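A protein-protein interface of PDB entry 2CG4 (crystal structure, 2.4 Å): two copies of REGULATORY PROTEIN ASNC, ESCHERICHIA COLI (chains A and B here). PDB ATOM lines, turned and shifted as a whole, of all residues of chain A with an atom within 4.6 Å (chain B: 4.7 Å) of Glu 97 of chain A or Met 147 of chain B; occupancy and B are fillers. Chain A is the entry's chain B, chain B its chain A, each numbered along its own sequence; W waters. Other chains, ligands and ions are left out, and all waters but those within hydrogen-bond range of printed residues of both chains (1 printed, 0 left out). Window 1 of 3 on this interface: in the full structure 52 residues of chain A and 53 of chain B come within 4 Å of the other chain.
NZ of Lys 110 of chain B sits at hydrogen-bond distance from OH of Tyr 99 of chain A, at 3.1 Å. The side-chain amide oxygen (OD1) of Asn 144 of chain B sits close to the backbone carbonyl oxygen (O) of Ala 98 of chain A, 3.0 Å away. The backbone carbonyl oxygen (O) of Ile 146 of chain B sits at hydrogen-bond distance from the backbone NH (N) of Ala 98 of chain A (2.9 Å). SD of Met 147 of chain B is in hydrogen-bond range of OH of Tyr 99 of chain A, 3.7 Å away. NE of Arg 148 of chain B is in hydrogen-bond range of O of Val 95 of chain A (2.9 Å). The backbone carbonyl oxygen (O) of Thr 96 of chain A is in hydrogen-bond range of the backbone NH (N) of Arg 148 of chain B, at 2.8 Å. The side-chain sulfur of Met 147 of chain B sits close to the side-chain carboxylate of Glu 97 of chain A (3.8 Å).
OD1 of Asn 144 of chain B lies close to O of Ile 146 of chain B (3.2 Å). N of Thr 96 of chain A is in hydrogen-bond range of O of Lys 110 of chain A (2.9 Å). The side-chain hydroxyl (OH) of Tyr 99 of chain A is in hydrogen-bond range of the side-chain carboxylate (OE1) of Glu 97 of chain A (2.7 Å). O of Glu 97 of chain A lies within hydrogen-bond range of N of Lys 110 of chain A, 3.0 Å away. The backbone NH (N) of Tyr 99 of chain A is in hydrogen-bond range of the backbone carbonyl oxygen (O) of Phe 108 of chain A (2.7 Å).
Among the printed residues, merely in contact across the chains: Thr 96 of chain A with Ile 146 of chain B (3.8 Å), Thr 96 of chain A with Met 147 of chain B (3.7 Å), Glu 97 of chain A with Ile 146 of chain B (3.2 Å), Ala 98 of chain A with Pro 145 of chain B (3.2 Å) and Tyr 99 of chain A with Asn 144 of chain B (3.2 Å).
Glu 97 of chain A touches two residues of chain B. Printed residues of chain B within 4 Å of Tyr 99 of chain A: Lys 110 (3.1 Å), Asn 144 (3.2 Å) and Met 147 (3.7 Å). Phe 108 of chain A touches none of the printed residues of chain B. Ile 109 of chain A touches none of the printed residues of chain B. Printed residues of chain A within 4 Å of Asn 144 of chain B: Ala 98 and Tyr 99. Of the printed residues of chain A, Pro 145 of chain B touches Ala 98. Met 147 of chain B touches just these residues of chain A: Thr 96, Glu 97 and Tyr 99. Of the printed residues of chain A, Arg 148 of chain B touches Val 95 (2.9 Å) and Thr 96 (2.8 Å). The nearest printed residue of chain A that does not touch Met 147 of chain B is Ala 98 of chain A (5.1 Å). The nearest printed residue of chain A that does not touch Arg 148 of chain B is Glu 97 of chain A (4.6 Å).
Of the 8 printed residues of chain A, 5 touch a printed residue of chain B. Printed residues of chain A that touch a printed residue of chain B: Val 95, Thr 96, Glu 97, Ala 98 and Tyr 99. Along chain A the printed residues that touch a printed residue of chain B span positions 95 to 99. Of the 6 printed residues of chain B, 6 touch a printed residue of chain A. Among the printed residues, 12 pairs touch across the chains. Among the printed residues, no Asp or Glu carboxylate lies within 4 Å of a Lys or Arg side-chain nitrogen of the other chain.
1 position is printed for both chains.
Water W1 lies within hydrogen-bond range of O of Arg 148 of chain B and OE2 of Glu 97 of chain A.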
ATOM      1  N   VAL A  95     -16.148  -8.751  19.471  1.00  0.00           N
ATOM      2  CA  VAL A  95     -15.130  -8.838  18.429  1.00  0.00           C
ATOM      3  C   VAL A  95     -13.766  -8.415  18.956  1.00  0.00           C
ATOM      4  O   VAL A  95     -13.514  -7.220  19.135  1.00  0.00           O
ATOM      5  CB  VAL A  95     -15.458  -7.916  17.255  1.00  0.00           C
ATOM      6  CG1 VAL A  95     -14.361  -7.995  16.198  1.00  0.00           C
ATOM      7  CG2 VAL A  95     -16.822  -8.247  16.659  1.00  0.00           C
ATOM      8  N   THR A  96     -12.882  -9.390  19.183  1.00  0.00           N
ATOM      9  CA  THR A  96     -11.551  -9.104  19.670  1.00  0.00           C
ATOM     10  C   THR A  96     -10.486  -8.887  18.576  1.00  0.00           C
ATOM     11  O   THR A  96      -9.439  -8.288  18.830  1.00  0.00           O
ATOM     12  CB  THR A  96     -11.093 -10.176  20.670  1.00  0.00           C
ATOM     13  OG1 THR A  96     -11.052 -11.460  20.032  1.00  0.00           O
ATOM     14  CG2 THR A  96     -12.052 -10.223  21.853  1.00  0.00           C
ATOM     15  N   GLU A  97     -10.743  -9.348  17.358  1.00  0.00           N
ATOM     16  CA  GLU A  97      -9.751  -9.226  16.299  1.00  0.00           C
ATOM     17  C   GLU A  97     -10.451  -9.160  14.964  1.00  0.00           C
ATOM     18  O   GLU A  97     -11.541  -9.680  14.812  1.00  0.00           O
ATOM     19  CB  GLU A  97      -8.816 -10.439  16.290  1.00  0.00           C
ATOM     20  CG  GLU A  97      -8.268 -10.819  17.638  1.00  0.00           C
ATOM     21  CD  GLU A  97      -7.234 -11.928  17.551  1.00  0.00           C
ATOM     22  OE1 GLU A  97      -7.131 -12.576  16.486  1.00  0.00           O
ATOM     23  OE2 GLU A  97      -6.522 -12.151  18.555  1.00  0.00           O
ATOM     24  N   ALA A  98      -9.816  -8.549  13.979  1.00  0.00           N
ATOM     25  CA  ALA A  98     -10.422  -8.493  12.655  1.00  0.00           C
ATOM     26  C   ALA A  98      -9.334  -8.366  11.630  1.00  0.00           C
ATOM     27  O   ALA A  98      -8.343  -7.665  11.853  1.00  0.00           O
ATOM     28  CB  ALA A  98     -11.420  -7.316  12.536  1.00  0.00           C
ATOM     29  N   TYR A  99      -9.516  -9.056  10.511  1.00  0.00           N
ATOM     30  CA  TYR A  99      -8.505  -9.111   9.484  1.00  0.00           C
ATOM     31  C   TYR A  99      -9.139  -8.942   8.123  1.00  0.00           C
ATOM     32  O   TYR A  99     -10.210  -9.493   7.843  1.00  0.00           O
ATOM     33  CB  TYR A  99      -7.786 -10.462   9.513  1.00  0.00           C
ATOM     34  CG  TYR A  99      -7.161 -10.818  10.838  1.00  0.00           C
ATOM     35  CD1 TYR A  99      -7.858 -11.580  11.773  1.00  0.00           C
ATOM     36  CD2 TYR A  99      -5.866 -10.402  11.156  1.00  0.00           C
ATOM     37  CE1 TYR A  99      -7.282 -11.931  12.993  1.00  0.00           C
ATOM     38  CE2 TYR A  99      -5.286 -10.747  12.367  1.00  0.00           C
ATOM     39  CZ  TYR A  99      -6.002 -11.509  13.281  1.00  0.00           C
ATOM     40  OH  TYR A  99      -5.433 -11.852  14.484  1.00  0.00           O
ATOM     41  N   PHE A 108     -12.426 -11.235   8.242  1.00  0.00           N
ATOM     42  CA  PHE A 108     -12.257 -12.427   9.061  1.00  0.00           C
ATOM     43  C   PHE A 108     -12.022 -11.959  10.500  1.00  0.00           C
ATOM     44  O   PHE A 108     -11.036 -11.283  10.789  1.00  0.00           O
ATOM     45  CB  PHE A 108     -11.078 -13.265   8.529  1.00  0.00           C
ATOM     46  CG  PHE A 108     -10.960 -14.635   9.149  1.00  0.00           C
ATOM     47  CD1 PHE A 108     -11.945 -15.598   8.944  1.00  0.00           C
ATOM     48  CD2 PHE A 108      -9.856 -14.971   9.927  1.00  0.00           C
ATOM     49  CE1 PHE A 108     -11.850 -16.862   9.518  1.00  0.00           C
ATOM     50  CE2 PHE A 108      -9.742 -16.244  10.500  1.00  0.00           C
ATOM     51  CZ  PHE A 108     -10.747 -17.187  10.293  1.00  0.00           C
ATOM     52  N   ILE A 109     -12.951 -12.289  11.389  1.00  0.00           N
ATOM     53  CA  ILE A 109     -12.967 -11.744  12.746  1.00  0.00           C
ATOM     54  C   ILE A 109     -12.941 -12.867  13.773  1.00  0.00           C
ATOM     55  O   ILE A 109     -13.341 -13.983  13.485  1.00  0.00           O
ATOM     56  CB  ILE A 109     -14.210 -10.839  13.010  1.00  0.00           C
ATOM     57  CG1 ILE A 109     -15.494 -11.668  13.035  1.00  0.00           C
ATOM     58  CG2 ILE A 109     -14.318  -9.733  11.970  1.00  0.00           C
ATOM     59  CD1 ILE A 109     -16.784 -10.826  13.225  1.00  0.00           C
ATOM     60  N   LYS A 110     -12.452 -12.558  14.970  1.00  0.00           N
ATOM     61  CA  LYS A 110     -12.643 -13.408  16.142  1.00  0.00           C
ATOM     62  C   LYS A 110     -13.677 -12.783  17.065  1.00  0.00           C
ATOM     63  O   LYS A 110     -13.558 -11.610  17.414  1.00  0.00           O
ATOM     64  CB  LYS A 110     -11.328 -13.583  16.899  1.00  0.00           C
ATOM     65  CG  LYS A 110     -11.175 -14.952  17.544  1.00  0.00           C
ATOM     66  CD  LYS A 110     -10.079 -14.956  18.586  1.00  0.00           C
ATOM     67  CE  LYS A 110      -9.525 -16.363  18.799  1.00  0.00           C
ATOM     68  NZ  LYS A 110      -8.330 -16.335  19.699  1.00  0.00           N
ATOM     69  N   LYS B 110      -2.240 -19.888  13.053  1.00  0.00           N
ATOM     70  CA  LYS B 110      -1.607 -18.642  12.644  1.00  0.00           C
ATOM     71  C   LYS B 110      -0.109 -18.835  12.531  1.00  0.00           C
ATOM     72  O   LYS B 110       0.511 -19.391  13.438  1.00  0.00           O
ATOM     73  CB  LYS B 110      -1.888 -17.552  13.664  1.00  0.00           C
ATOM     74  CG  LYS B 110      -2.099 -16.202  13.060  1.00  0.00           C
ATOM     75  CD  LYS B 110      -1.975 -15.139  14.119  1.00  0.00           C
ATOM     76  CE  LYS B 110      -2.515 -13.797  13.626  1.00  0.00           C
ATOM     77  NZ  LYS B 110      -2.542 -12.821  14.755  1.00  0.00           N
ATOM     78  N   ASN B 144      -4.786  -5.741   9.432  1.00  0.00           N
ATOM     79  CA  ASN B 144      -5.249  -6.231  10.729  1.00  0.00           C
ATOM     80  C   ASN B 144      -5.726  -5.114  11.647  1.00  0.00           C
ATOM     81  O   ASN B 144      -5.093  -4.854  12.664  1.00  0.00           O
ATOM     82  CB  ASN B 144      -4.128  -7.000  11.437  1.00  0.00           C
ATOM     83  CG  ASN B 144      -4.482  -7.358  12.870  1.00  0.00           C
ATOM     84  OD1 ASN B 144      -5.627  -7.686  13.178  1.00  0.00           O
ATOM     85  ND2 ASN B 144      -3.505  -7.290  13.750  1.00  0.00           N
ATOM     86  N   PRO B 145      -6.853  -4.463  11.301  1.00  0.00           N
ATOM     87  CA  PRO B 145      -7.299  -3.201  11.901  1.00  0.00           C
ATOM     88  C   PRO B 145      -7.717  -3.286  13.382  1.00  0.00           C
ATOM     89  O   PRO B 145      -7.459  -2.349  14.148  1.00  0.00           O
ATOM     90  CB  PRO B 145      -8.511  -2.819  11.046  1.00  0.00           C
ATOM     91  CG  PRO B 145      -9.018  -4.124  10.489  1.00  0.00           C
ATOM     92  CD  PRO B 145      -7.791  -4.948  10.267  1.00  0.00           C
ATOM     93  N   ILE B 146      -8.383  -4.373  13.772  1.00  0.00           N
ATOM     94  CA  ILE B 146      -8.754  -4.599  15.171  1.00  0.00           C
ATOM     95  C   ILE B 146      -7.869  -5.698  15.771  1.00  0.00           C
ATOM     96  O   ILE B 146      -7.854  -6.830  15.303  1.00  0.00           O
ATOM     97  CB  ILE B 146     -10.229  -4.992  15.313  1.00  0.00           C
ATOM     98  CG1 ILE B 146     -11.144  -3.861  14.816  1.00  0.00           C
ATOM     99  CG2 ILE B 146     -10.551  -5.332  16.775  1.00  0.00           C
ATOM    100  CD1 ILE B 146     -12.605  -4.274  14.610  1.00  0.00           C
ATOM    101  N   MET B 147      -7.107  -5.343  16.795  1.00  0.00           N
ATOM    102  CA  MET B 147      -6.549  -6.339  17.679  1.00  0.00           C
ATOM    103  C   MET B 147      -6.658  -5.871  19.118  1.00  0.00           C
ATOM    104  O   MET B 147      -6.051  -4.874  19.516  1.00  0.00           O
ATOM    105  CB  MET B 147      -5.109  -6.688  17.297  1.00  0.00           C
ATOM    106  CG  MET B 147      -5.026  -7.848  16.297  1.00  0.00           C
ATOM    107  SD  MET B 147      -4.430  -9.405  17.005  1.00  0.00           S
ATOM    108  CE  MET B 147      -4.935  -9.233  18.718  1.00  0.00           C
ATOM    109  N   ARG B 148      -7.458  -6.598  19.888  1.00  0.00           N
ATOM    110  CA  ARG B 148      -7.642  -6.290  21.287  1.00  0.00           C
ATOM    111  C   ARG B 148      -8.014  -7.549  22.050  1.00  0.00           C
ATOM    112  O   ARG B 148      -7.659  -8.663  21.660  1.00  0.00           O
ATOM    113  CB  ARG B 148      -8.729  -5.228  21.451  1.00  0.00           C
ATOM    114  CG  ARG B 148     -10.078  -5.638  20.870  1.00  0.00           C
ATOM    115  CD  ARG B 148     -10.985  -4.450  20.662  1.00  0.00           C
ATOM    116  NE  ARG B 148     -12.226  -4.827  20.004  1.00  0.00           N
ATOM    117  CZ  ARG B 148     -13.032  -3.961  19.386  1.00  0.00           C
ATOM    118  NH1 ARG B 148     -12.705  -2.682  19.344  1.00  0.00           N
ATOM    119  NH2 ARG B 148     -14.162  -4.370  18.805  1.00  0.00           N
HETATM  120  O   HOH W   1      -6.527 -10.924  21.018  1.00  0.00           O
